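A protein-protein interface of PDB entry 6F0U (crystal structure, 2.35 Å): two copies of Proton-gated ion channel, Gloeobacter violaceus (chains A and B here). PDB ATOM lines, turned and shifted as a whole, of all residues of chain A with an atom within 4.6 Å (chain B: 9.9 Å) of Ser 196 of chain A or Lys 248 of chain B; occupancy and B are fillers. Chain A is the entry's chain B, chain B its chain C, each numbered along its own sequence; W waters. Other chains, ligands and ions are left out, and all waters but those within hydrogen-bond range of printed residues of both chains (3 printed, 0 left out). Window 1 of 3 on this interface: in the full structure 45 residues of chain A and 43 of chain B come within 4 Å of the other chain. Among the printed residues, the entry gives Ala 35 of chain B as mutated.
The side-chain hydroxyl (OH) of Tyr 119 of chain A lies within hydrogen-bond range of the side-chain hydroxyl (OH) of Tyr 197 of chain A (3.1 Å).
OE1 of Glu 243 of chain B lies close to OD1 of Asn 239 of chain B (3.3 Å).
NZ of Lys 33 of chain B is in hydrogen-bond range of O of Glu 243 of chain B, 3.4 Å away.
The side-chain amino group (NZ) of Lys 33 of chain B lies within hydrogen-bond range of the backbone carbonyl oxygen (O) of Leu 246 of chain B.
The side-chain hydroxyl (OG1) of Thr 249 of chain B is in hydrogen-bond range of the backbone carbonyl oxygen (O) of Tyr 251 of chain B (2.9 Å).
N of Phe 116 of chain B lies within hydrogen-bond range of OH of Tyr 251 of chain B (2.7 Å).
Among the printed residues, merely in contact across the chains: Tyr 119 of chain A with Lys 248 of chain B (3.9 Å), Thr 158 of chain A with Lys 33 of chain B (3.8 Å), Thr 158 of chain A with Pro 247 of chain B (3.8 Å), Gln 193 of chain A with Pro 250 of chain B (3.4 Å), Phe 195 of chain A with Thr 249 of chain B (3.3 Å), Phe 195 of chain A with Pro 250 of chain B (3.7 Å), Phe 195 of chain A with Tyr 251 of chain B (3.3 Å), Phe 195 of chain A with Met 252 of chain B (3.7 Å), Ser 196 of chain A with Lys 248 of chain B (3.3 Å), Ser 196 of chain A with Thr 249 of chain B (3.6 Å), Pro 199 of chain A with Met 252 of chain B (3.8 Å), Pro 199 of chain A with Phe 260 of chain B (3.6 Å), Asn 200 of chain A with Asn 239 of chain B (3.8 Å) and Asn 200 of chain A with Glu 243 of chain B (3.5 Å).
Of the 22 printed residues of chain B, 10 touch a printed residue of chain A.
Printed residues of chain A that touch a printed residue of chain B: Tyr 119, Thr 158, Gln 193, Phe 195, Ser 196, Tyr 197, Pro 199, Asn 200 and Asn 245.
Among the printed residues, no Asp or Glu carboxylate lies within 4 Å of a Lys or Arg side-chain nitrogen of the other chain.
OH of Tyr 197 of chain A lies within hydrogen-bond range of NZ of Lys 248 of chain B (3.0 Å).
OD1 of Asn 245 of chain A sits at hydrogen-bond distance from NZ of Lys 248 of chain B, at 3.4 Å.
1 position is printed for both chains.
Of the 16 pairs that touch across the chains among the printed residues, none has its exchanged pair printed and touching as well.
Water W2 bridges O of Pro 199 of chain A (2.6 Å) and ND2 of Asn 239 of chain B (2.8 Å).
Water W3 lies within hydrogen-bond range of OE1 of Gln 193 of chain A (2.7 Å) and O of Lys 248 of chain B (2.9 Å).
Water W1 lies within hydrogen-bond range of O of Gly 256 of chain B and OD1 of Asn 200 of chain A.
Of chain B, only Lys 248 (3.3 Å) and Thr 249 (3.6 Å) come within 4 Å of Ser 196 of chain A.
Lys 248 of chain B touches four residues of chain A.
Of chain B, only Thr 249 (3.3 Å), Pro 250 (3.7 Å), Tyr 251 (3.3 Å) and Met 252 (3.7 Å) come within 4 Å of Phe 195 of chain A.
Asn 200 of chain A touches two residues of chain B.
Of the printed residues of chain B, Asn 245 of chain A touches Lys 248 (3.4 Å).
Printed residues of chain A within 4 Å of Asn 239 of chain B: Asn 200.
The nearest printed residue of chain A that does not touch Met 252 of chain B is Ser 196 of chain A (6.6 Å).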
ATOM      1  N   TYR A 119      17.947 -32.943   9.862  1.00  0.00           N
ATOM      2  CA  TYR A 119      18.644 -32.148   8.855  1.00  0.00           C
ATOM      3  C   TYR A 119      20.184 -32.172   9.032  1.00  0.00           C
ATOM      4  O   TYR A 119      20.662 -32.008  10.161  1.00  0.00           O
ATOM      5  CB  TYR A 119      18.125 -30.710   8.894  1.00  0.00           C
ATOM      6  CG  TYR A 119      18.768 -29.774   7.895  1.00  0.00           C
ATOM      7  CD1 TYR A 119      19.879 -29.007   8.238  1.00  0.00           C
ATOM      8  CD2 TYR A 119      18.224 -29.602   6.631  1.00  0.00           C
ATOM      9  CE1 TYR A 119      20.438 -28.103   7.340  1.00  0.00           C
ATOM     10  CE2 TYR A 119      18.778 -28.705   5.725  1.00  0.00           C
ATOM     11  CZ  TYR A 119      19.883 -27.958   6.081  1.00  0.00           C
ATOM     12  OH  TYR A 119      20.400 -27.062   5.179  1.00  0.00           O
ATOM     13  N   THR A 158      16.368 -30.566  -7.298  1.00  0.00           N
ATOM     14  CA  THR A 158      17.718 -30.156  -6.916  1.00  0.00           C
ATOM     15  C   THR A 158      17.949 -30.335  -5.410  1.00  0.00           C
ATOM     16  O   THR A 158      17.190 -29.802  -4.604  1.00  0.00           O
ATOM     17  CB  THR A 158      17.998 -28.713  -7.407  1.00  0.00           C
ATOM     18  OG1 THR A 158      17.744 -28.613  -8.811  1.00  0.00           O
ATOM     19  CG2 THR A 158      19.420 -28.245  -7.096  1.00  0.00           C
ATOM     20  N   GLY A 159      18.975 -31.113  -5.068  1.00  0.00           N
ATOM     21  CA  GLY A 159      19.355 -31.409  -3.690  1.00  0.00           C
ATOM     22  C   GLY A 159      18.571 -32.528  -3.026  1.00  0.00           C
ATOM     23  O   GLY A 159      18.701 -32.741  -1.819  1.00  0.00           O
ATOM     24  N   GLN A 193      19.867 -35.080  -0.255  1.00  0.00           N
ATOM     25  CA  GLN A 193      21.219 -35.402  -0.666  1.00  0.00           C
ATOM     26  C   GLN A 193      22.121 -34.586   0.263  1.00  0.00           C
ATOM     27  O   GLN A 193      22.357 -33.390   0.040  1.00  0.00           O
ATOM     28  CB  GLN A 193      21.458 -35.060  -2.152  1.00  0.00           C
ATOM     29  CG  GLN A 193      20.629 -35.913  -3.087  1.00  0.00           C
ATOM     30  CD  GLN A 193      20.770 -35.557  -4.538  1.00  0.00           C
ATOM     31  OE1 GLN A 193      21.079 -34.422  -4.919  1.00  0.00           O
ATOM     32  NE2 GLN A 193      20.469 -36.521  -5.382  1.00  0.00           N
ATOM     33  N   TYR A 194      22.556 -35.230   1.349  1.00  0.00           N
ATOM     34  CA  TYR A 194      23.429 -34.642   2.385  1.00  0.00           C
ATOM     35  C   TYR A 194      24.890 -34.412   1.977  1.00  0.00           C
ATOM     36  O   TYR A 194      25.570 -33.628   2.643  1.00  0.00           O
ATOM     37  CB  TYR A 194      23.392 -35.488   3.662  1.00  0.00           C
ATOM     38  CG  TYR A 194      23.749 -36.939   3.433  1.00  0.00           C
ATOM     39  CD1 TYR A 194      25.078 -37.347   3.349  1.00  0.00           C
ATOM     40  CD2 TYR A 194      22.758 -37.910   3.330  1.00  0.00           C
ATOM     41  CE1 TYR A 194      25.413 -38.682   3.156  1.00  0.00           C
ATOM     42  CE2 TYR A 194      23.080 -39.251   3.139  1.00  0.00           C
ATOM     43  CZ  TYR A 194      24.409 -39.630   3.045  1.00  0.00           C
ATOM     44  OH  TYR A 194      24.730 -40.947   2.845  1.00  0.00           O
ATOM     45  N   PHE A 195      25.373 -35.116   0.918  1.00  0.00           N
ATOM     46  CA  PHE A 195      26.741 -35.056   0.388  1.00  0.00           C
ATOM     47  C   PHE A 195      27.422 -33.706   0.549  1.00  0.00           C
ATOM     48  O   PHE A 195      28.451 -33.633   1.212  1.00  0.00           O
ATOM     49  CB  PHE A 195      26.810 -35.507  -1.099  1.00  0.00           C
ATOM     50  CG  PHE A 195      28.201 -35.402  -1.706  1.00  0.00           C
ATOM     51  CD1 PHE A 195      28.671 -34.194  -2.218  1.00  0.00           C
ATOM     52  CD2 PHE A 195      29.060 -36.489  -1.705  1.00  0.00           C
ATOM     53  CE1 PHE A 195      29.973 -34.078  -2.704  1.00  0.00           C
ATOM     54  CE2 PHE A 195      30.367 -36.371  -2.202  1.00  0.00           C
ATOM     55  CZ  PHE A 195      30.806 -35.172  -2.716  1.00  0.00           C
ATOM     56  N   SER A 196      26.884 -32.661  -0.115  1.00  0.00           N
ATOM     57  CA  SER A 196      27.442 -31.300  -0.181  1.00  0.00           C
ATOM     58  C   SER A 196      27.727 -30.678   1.168  1.00  0.00           C
ATOM     59  O   SER A 196      28.677 -29.927   1.295  1.00  0.00           O
ATOM     60  CB  SER A 196      26.550 -30.380  -1.017  1.00  0.00           C
ATOM     61  OG  SER A 196      25.225 -30.412  -0.516  1.00  0.00           O
ATOM     62  N   TYR A 197      26.892 -30.971   2.165  1.00  0.00           N
ATOM     63  CA  TYR A 197      27.028 -30.423   3.507  1.00  0.00           C
ATOM     64  C   TYR A 197      28.330 -30.812   4.172  1.00  0.00           C
ATOM     65  O   TYR A 197      28.831 -30.055   4.990  1.00  0.00           O
ATOM     66  CB  TYR A 197      25.839 -30.841   4.367  1.00  0.00           C
ATOM     67  CG  TYR A 197      24.543 -30.239   3.895  1.00  0.00           C
ATOM     68  CD1 TYR A 197      23.788 -30.847   2.894  1.00  0.00           C
ATOM     69  CD2 TYR A 197      24.078 -29.048   4.425  1.00  0.00           C
ATOM     70  CE1 TYR A 197      22.595 -30.282   2.439  1.00  0.00           C
ATOM     71  CE2 TYR A 197      22.879 -28.483   3.989  1.00  0.00           C
ATOM     72  CZ  TYR A 197      22.139 -29.106   2.997  1.00  0.00           C
ATOM     73  OH  TYR A 197      20.957 -28.548   2.574  1.00  0.00           O
ATOM     74  N   ILE A 198      28.867 -31.972   3.831  1.00  0.00           N
ATOM     75  CA  ILE A 198      30.113 -32.468   4.385  1.00  0.00           C
ATOM     76  C   ILE A 198      31.323 -31.583   4.020  1.00  0.00           C
ATOM     77  O   ILE A 198      31.913 -31.006   4.928  1.00  0.00           O
ATOM     78  CB  ILE A 198      30.301 -33.939   4.007  1.00  0.00           C
ATOM     79  CG1 ILE A 198      29.138 -34.772   4.585  1.00  0.00           C
ATOM     80  CG2 ILE A 198      31.650 -34.423   4.504  1.00  0.00           C
ATOM     81  CD1 ILE A 198      28.990 -36.085   4.014  1.00  0.00           C
ATOM     82  N   PRO A 199      31.671 -31.407   2.715  1.00  0.00           N
ATOM     83  CA  PRO A 199      32.798 -30.515   2.361  1.00  0.00           C
ATOM     84  C   PRO A 199      32.502 -29.022   2.569  1.00  0.00           C
ATOM     85  O   PRO A 199      33.435 -28.244   2.697  1.00  0.00           O
ATOM     86  CB  PRO A 199      33.013 -30.788   0.866  1.00  0.00           C
ATOM     87  CG  PRO A 199      31.718 -31.351   0.386  1.00  0.00           C
ATOM     88  CD  PRO A 199      31.105 -32.064   1.516  1.00  0.00           C
ATOM     89  N   ASN A 200      31.217 -28.610   2.517  1.00  0.00           N
ATOM     90  CA  ASN A 200      30.871 -27.181   2.599  1.00  0.00           C
ATOM     91  C   ASN A 200      30.628 -26.616   3.985  1.00  0.00           C
ATOM     92  O   ASN A 200      30.895 -25.429   4.194  1.00  0.00           O
ATOM     93  CB  ASN A 200      29.674 -26.869   1.722  1.00  0.00           C
ATOM     94  CG  ASN A 200      29.998 -26.957   0.254  1.00  0.00           C
ATOM     95  OD1 ASN A 200      31.012 -26.428  -0.231  1.00  0.00           O
ATOM     96  ND2 ASN A 200      29.117 -27.595  -0.488  1.00  0.00           N
ATOM     97  N   ASN A 245      19.448 -21.089   5.554  1.00  0.00           N
ATOM     98  CA  ASN A 245      18.914 -22.176   4.723  1.00  0.00           C
ATOM     99  C   ASN A 245      17.787 -22.932   5.438  1.00  0.00           C
ATOM    100  O   ASN A 245      17.134 -23.781   4.837  1.00  0.00           O
ATOM    101  CB  ASN A 245      20.040 -23.181   4.340  1.00  0.00           C
ATOM    102  CG  ASN A 245      21.280 -22.615   3.663  1.00  0.00           C
ATOM    103  OD1 ASN A 245      22.390 -23.139   3.826  1.00  0.00           O
ATOM    104  ND2 ASN A 245      21.129 -21.559   2.866  1.00  0.00           N
ATOM    105  N   ASP B  32      21.357 -20.925 -12.625  1.00  0.00           N
ATOM    106  CA  ASP B  32      22.203 -22.093 -12.331  1.00  0.00           C
ATOM    107  C   ASP B  32      21.671 -22.929 -11.147  1.00  0.00           C
ATOM    108  O   ASP B  32      21.563 -24.148 -11.265  1.00  0.00           O
ATOM    109  CB  ASP B  32      23.654 -21.632 -12.020  1.00  0.00           C
ATOM    110  CG  ASP B  32      24.493 -21.279 -13.234  1.00  0.00           C
ATOM    111  OD1 ASP B  32      24.401 -20.125 -13.710  1.00  0.00           O
ATOM    112  OD2 ASP B  32      25.268 -22.134 -13.680  1.00  0.00           O
ATOM    113  N   LYS B  33      21.360 -22.271 -10.011  1.00  0.00           N
ATOM    114  CA  LYS B  33      20.862 -22.925  -8.798  1.00  0.00           C
ATOM    115  C   LYS B  33      19.525 -23.619  -9.043  1.00  0.00           C
ATOM    116  O   LYS B  33      19.341 -24.764  -8.608  1.00  0.00           O
ATOM    117  CB  LYS B  33      20.728 -21.925  -7.628  1.00  0.00           C
ATOM    118  CG  LYS B  33      22.044 -21.535  -6.956  1.00  0.00           C
ATOM    119  CD  LYS B  33      21.874 -20.400  -5.918  1.00  0.00           C
ATOM    120  CE  LYS B  33      21.648 -20.879  -4.497  1.00  0.00           C
ATOM    121  NZ  LYS B  33      22.885 -21.426  -3.854  1.00  0.00           N
ATOM    122  N   ALA B  34      18.609 -22.930  -9.759  1.00  0.00           N
ATOM    123  CA  ALA B  34      17.257 -23.396 -10.087  1.00  0.00           C
ATOM    124  C   ALA B  34      17.151 -24.384 -11.247  1.00  0.00           C
ATOM    125  O   ALA B  34      16.120 -25.048 -11.345  1.00  0.00           O
ATOM    126  CB  ALA B  34      16.352 -22.206 -10.353  1.00  0.00           C
ATOM    127  N   ALA B  35      18.179 -24.468 -12.143  1.00  0.00           N
ATOM    128  CA  ALA B  35      18.200 -25.297 -13.361  1.00  0.00           C
ATOM    129  C   ALA B  35      17.082 -24.826 -14.317  1.00  0.00           C
ATOM    130  O   ALA B  35      16.407 -25.638 -14.961  1.00  0.00           O
ATOM    131  CB  ALA B  35      18.032 -26.780 -13.015  1.00  0.00           C
ATOM    132  N   LEU B 114      21.684 -29.056 -14.855  1.00  0.00           N
ATOM    133  CA  LEU B 114      23.048 -28.728 -15.243  1.00  0.00           C
ATOM    134  C   LEU B 114      24.054 -29.588 -14.496  1.00  0.00           C
ATOM    135  O   LEU B 114      23.821 -29.962 -13.342  1.00  0.00           O
ATOM    136  CB  LEU B 114      23.336 -27.226 -15.007  1.00  0.00           C
ATOM    137  CG  LEU B 114      22.244 -26.243 -15.462  1.00  0.00           C
ATOM    138  CD1 LEU B 114      22.432 -24.905 -14.834  1.00  0.00           C
ATOM    139  CD2 LEU B 114      22.283 -26.061 -16.923  1.00  0.00           C
ATOM    140  N   PHE B 116      27.547 -29.581 -12.846  1.00  0.00           N
ATOM    141  CA  PHE B 116      28.507 -28.625 -12.287  1.00  0.00           C
ATOM    142  C   PHE B 116      29.923 -29.176 -11.996  1.00  0.00           C
ATOM    143  O   PHE B 116      30.776 -28.409 -11.532  1.00  0.00           O
ATOM    144  CB  PHE B 116      27.918 -27.965 -11.030  1.00  0.00           C
ATOM    145  CG  PHE B 116      26.751 -27.059 -11.317  1.00  0.00           C
ATOM    146  CD1 PHE B 116      26.955 -25.729 -11.688  1.00  0.00           C
ATOM    147  CD2 PHE B 116      25.444 -27.528 -11.218  1.00  0.00           C
ATOM    148  CE1 PHE B 116      25.869 -24.890 -11.954  1.00  0.00           C
ATOM    149  CE2 PHE B 116      24.366 -26.689 -11.489  1.00  0.00           C
ATOM    150  CZ  PHE B 116      24.587 -25.377 -11.852  1.00  0.00           C
ATOM    151  N   ASN B 239      34.794 -19.336   0.094  1.00  0.00           N
ATOM    152  CA  ASN B 239      34.033 -20.593   0.076  1.00  0.00           C
ATOM    153  C   ASN B 239      32.520 -20.264   0.139  1.00  0.00           C
ATOM    154  O   ASN B 239      31.751 -20.799  -0.654  1.00  0.00           O
ATOM    155  CB  ASN B 239      34.423 -21.506   1.269  1.00  0.00           C
ATOM    156  CG  ASN B 239      33.767 -22.885   1.244  1.00  0.00           C
ATOM    157  OD1 ASN B 239      33.044 -23.262   0.304  1.00  0.00           O
ATOM    158  ND2 ASN B 239      33.994 -23.682   2.280  1.00  0.00           N
ATOM    159  N   ILE B 240      32.111 -19.369   1.075  1.00  0.00           N
ATOM    160  CA  ILE B 240      30.717 -18.969   1.227  1.00  0.00           C
ATOM    161  C   ILE B 240      30.214 -18.285  -0.032  1.00  0.00           C
ATOM    162  O   ILE B 240      29.139 -18.627  -0.503  1.00  0.00           O
ATOM    163  CB  ILE B 240      30.467 -18.147   2.514  1.00  0.00           C
ATOM    164  CG1 ILE B 240      30.792 -19.012   3.763  1.00  0.00           C
ATOM    165  CG2 ILE B 240      28.980 -17.612   2.539  1.00  0.00           C
ATOM    166  CD1 ILE B 240      30.825 -18.296   5.099  1.00  0.00           C
ATOM    167  N   VAL B 242      31.303 -18.631  -3.148  1.00  0.00           N
ATOM    168  CA  VAL B 242      31.202 -19.626  -4.206  1.00  0.00           C
ATOM    169  C   VAL B 242      29.929 -20.468  -4.036  1.00  0.00           C
ATOM    170  O   VAL B 242      29.174 -20.619  -5.002  1.00  0.00           O
ATOM    171  CB  VAL B 242      32.502 -20.476  -4.335  1.00  0.00           C
ATOM    172  CG1 VAL B 242      32.295 -21.696  -5.242  1.00  0.00           C
ATOM    173  CG2 VAL B 242      33.661 -19.619  -4.840  1.00  0.00           C
ATOM    174  N   GLU B 243      29.669 -20.975  -2.818  1.00  0.00           N
ATOM    175  CA  GLU B 243      28.509 -21.839  -2.624  1.00  0.00           C
ATOM    176  C   GLU B 243      27.159 -21.076  -2.737  1.00  0.00           C
ATOM    177  O   GLU B 243      26.146 -21.732  -2.993  1.00  0.00           O
ATOM    178  CB  GLU B 243      28.606 -22.723  -1.364  1.00  0.00           C
ATOM    179  CG  GLU B 243      28.704 -22.051  -0.013  1.00  0.00           C
ATOM    180  CD  GLU B 243      28.844 -23.064   1.110  1.00  0.00           C
ATOM    181  OE1 GLU B 243      29.985 -23.297   1.567  1.00  0.00           O
ATOM    182  OE2 GLU B 243      27.817 -23.664   1.499  1.00  0.00           O
ATOM    183  N   THR B 244      27.155 -19.719  -2.694  1.00  0.00           N
ATOM    184  CA  THR B 244      25.937 -18.923  -2.926  1.00  0.00           C
ATOM    185  C   THR B 244      25.579 -18.865  -4.420  1.00  0.00           C
ATOM    186  O   THR B 244      24.417 -18.654  -4.741  1.00  0.00           O
ATOM    187  CB  THR B 244      25.995 -17.501  -2.315  1.00  0.00           C
ATOM    188  OG1 THR B 244      26.989 -16.703  -2.959  1.00  0.00           O
ATOM    189  CG2 THR B 244      26.160 -17.496  -0.816  1.00  0.00           C
ATOM    190  N   ASN B 245      26.567 -19.039  -5.322  1.00  0.00           N
ATOM    191  CA  ASN B 245      26.387 -19.038  -6.788  1.00  0.00           C
ATOM    192  C   ASN B 245      26.116 -20.451  -7.333  1.00  0.00           C
ATOM    193  O   ASN B 245      25.806 -20.609  -8.518  1.00  0.00           O
ATOM    194  CB  ASN B 245      27.635 -18.463  -7.503  1.00  0.00           C
ATOM    195  CG  ASN B 245      28.105 -17.088  -7.084  1.00  0.00           C
ATOM    196  OD1 ASN B 245      29.301 -16.783  -7.154  1.00  0.00           O
ATOM    197  ND2 ASN B 245      27.192 -16.213  -6.670  1.00  0.00           N
ATOM    198  N   LEU B 246      26.252 -21.472  -6.476  1.00  0.00           N
ATOM    199  CA  LEU B 246      26.094 -22.867  -6.855  1.00  0.00           C
ATOM    200  C   LEU B 246      25.009 -23.600  -6.092  1.00  0.00           C
ATOM    201  O   LEU B 246      24.847 -23.360  -4.899  1.00  0.00           O
ATOM    202  CB  LEU B 246      27.414 -23.609  -6.609  1.00  0.00           C
ATOM    203  CG  LEU B 246      28.541 -23.392  -7.598  1.00  0.00           C
ATOM    204  CD1 LEU B 246      29.777 -24.106  -7.140  1.00  0.00           C
ATOM    205  CD2 LEU B 246      28.168 -23.893  -8.977  1.00  0.00           C
ATOM    206  N   PRO B 247      24.317 -24.579  -6.713  1.00  0.00           N
ATOM    207  CA  PRO B 247      23.366 -25.389  -5.940  1.00  0.00           C
ATOM    208  C   PRO B 247      24.116 -26.476  -5.149  1.00  0.00           C
ATOM    209  O   PRO B 247      25.289 -26.706  -5.378  1.00  0.00           O
ATOM    210  CB  PRO B 247      22.505 -26.024  -7.034  1.00  0.00           C
ATOM    211  CG  PRO B 247      23.455 -26.230  -8.139  1.00  0.00           C
ATOM    212  CD  PRO B 247      24.366 -25.031  -8.122  1.00  0.00           C
ATOM    213  N   LYS B 248      23.430 -27.152  -4.245  1.00  0.00           N
ATOM    214  CA  LYS B 248      23.973 -28.265  -3.482  1.00  0.00           C
ATOM    215  C   LYS B 248      23.996 -29.494  -4.403  1.00  0.00           C
ATOM    216  O   LYS B 248      22.946 -29.921  -4.886  1.00  0.00           O
ATOM    217  CB  LYS B 248      23.126 -28.486  -2.217  1.00  0.00           C
ATOM    218  CG  LYS B 248      23.466 -27.449  -1.166  1.00  0.00           C
ATOM    219  CD  LYS B 248      22.402 -27.233  -0.124  1.00  0.00           C
ATOM    220  CE  LYS B 248      22.833 -26.073   0.744  1.00  0.00           C
ATOM    221  NZ  LYS B 248      21.893 -25.813   1.852  1.00  0.00           N
ATOM    222  N   THR B 249      25.200 -30.019  -4.698  1.00  0.00           N
ATOM    223  CA  THR B 249      25.348 -31.169  -5.625  1.00  0.00           C
ATOM    224  C   THR B 249      25.704 -32.499  -4.920  1.00  0.00           C
ATOM    225  O   THR B 249      26.475 -32.488  -3.957  1.00  0.00           O
ATOM    226  CB  THR B 249      26.355 -30.833  -6.726  1.00  0.00           C
ATOM    227  OG1 THR B 249      27.581 -30.403  -6.109  1.00  0.00           O
ATOM    228  CG2 THR B 249      25.840 -29.773  -7.683  1.00  0.00           C
ATOM    229  N   PRO B 250      25.195 -33.666  -5.395  1.00  0.00           N
ATOM    230  CA  PRO B 250      25.558 -34.938  -4.727  1.00  0.00           C
ATOM    231  C   PRO B 250      26.936 -35.458  -5.189  1.00  0.00           C
ATOM    232  O   PRO B 250      27.273 -36.633  -5.028  1.00  0.00           O
ATOM    233  CB  PRO B 250      24.401 -35.872  -5.125  1.00  0.00           C
ATOM    234  CG  PRO B 250      23.968 -35.375  -6.479  1.00  0.00           C
ATOM    235  CD  PRO B 250      24.284 -33.901  -6.549  1.00  0.00           C
ATOM    236  N   TYR B 251      27.726 -34.568  -5.779  1.00  0.00           N
ATOM    237  CA  TYR B 251      29.053 -34.840  -6.301  1.00  0.00           C
ATOM    238  C   TYR B 251      29.929 -33.653  -5.999  1.00  0.00           C
ATOM    239  O   TYR B 251      29.408 -32.574  -5.681  1.00  0.00           O
ATOM    240  CB  TYR B 251      29.011 -35.098  -7.831  1.00  0.00           C
ATOM    241  CG  TYR B 251      28.305 -34.033  -8.644  1.00  0.00           C
ATOM    242  CD1 TYR B 251      28.941 -32.833  -8.965  1.00  0.00           C
ATOM    243  CD2 TYR B 251      27.007 -34.231  -9.112  1.00  0.00           C
ATOM    244  CE1 TYR B 251      28.286 -31.840  -9.694  1.00  0.00           C
ATOM    245  CE2 TYR B 251      26.344 -33.251  -9.846  1.00  0.00           C
ATOM    246  CZ  TYR B 251      26.992 -32.058 -10.144  1.00  0.00           C
ATOM    247  OH  TYR B 251      26.363 -31.081 -10.874  1.00  0.00           O
ATOM    248  N   MET B 252      31.257 -33.830  -6.143  1.00  0.00           N
ATOM    249  CA  MET B 252      32.195 -32.746  -5.948  1.00  0.00           C
ATOM    250  C   MET B 252      32.357 -31.945  -7.257  1.00  0.00           C
ATOM    251  O   MET B 252      32.399 -32.539  -8.330  1.00  0.00           O
ATOM    252  CB  MET B 252      33.556 -33.301  -5.484  1.00  0.00           C
ATOM    253  CG  MET B 252      34.210 -32.447  -4.446  1.00  0.00           C
ATOM    254  SD  MET B 252      33.333 -32.472  -2.845  1.00  0.00           S
ATOM    255  CE  MET B 252      34.131 -33.763  -2.101  1.00  0.00           C
ATOM    256  N   THR B 253      32.431 -30.610  -7.166  1.00  0.00           N
ATOM    257  CA  THR B 253      32.713 -29.769  -8.330  1.00  0.00           C
ATOM    258  C   THR B 253      34.236 -29.518  -8.344  1.00  0.00           C
ATOM    259  O   THR B 253      34.913 -29.776  -7.333  1.00  0.00           O
ATOM    260  CB  THR B 253      31.900 -28.460  -8.313  1.00  0.00           C
ATOM    261  OG1 THR B 253      32.320 -27.635  -7.232  1.00  0.00           O
ATOM    262  CG2 THR B 253      30.394 -28.700  -8.262  1.00  0.00           C
ATOM    263  N   GLY B 256      34.900 -26.612  -5.948  1.00  0.00           N
ATOM    264  CA  GLY B 256      34.589 -27.161  -4.638  1.00  0.00           C
ATOM    265  C   GLY B 256      35.715 -28.001  -4.077  1.00  0.00           C
ATOM    266  O   GLY B 256      36.020 -27.893  -2.895  1.00  0.00           O
ATOM    267  N   PHE B 260      38.000 -27.026  -0.950  1.00  0.00           N
ATOM    268  CA  PHE B 260      38.076 -27.970   0.164  1.00  0.00           C
ATOM    269  C   PHE B 260      39.533 -28.345   0.513  1.00  0.00           C
ATOM    270  O   PHE B 260      39.905 -28.363   1.684  1.00  0.00           O
ATOM    271  CB  PHE B 260      37.215 -29.227  -0.089  1.00  0.00           C
ATOM    272  CG  PHE B 260      37.308 -30.178   1.075  1.00  0.00           C
ATOM    273  CD1 PHE B 260      36.625 -29.921   2.258  1.00  0.00           C
ATOM    274  CD2 PHE B 260      38.161 -31.277   1.029  1.00  0.00           C
ATOM    275  CE1 PHE B 260      36.775 -30.754   3.362  1.00  0.00           C
ATOM    276  CE2 PHE B 260      38.321 -32.105   2.140  1.00  0.00           C
ATOM    277  CZ  PHE B 260      37.632 -31.835   3.300  1.00  0.00           C
HETATM  278  O   HOH W   1      34.149 -27.374  -0.957  1.00  0.00           O
HETATM  279  O   HOH W   2      34.635 -26.260   1.459  1.00  0.00           O
HETATM  280  O   HOH W   3      22.536 -32.526  -3.626  1.00  0.00           O
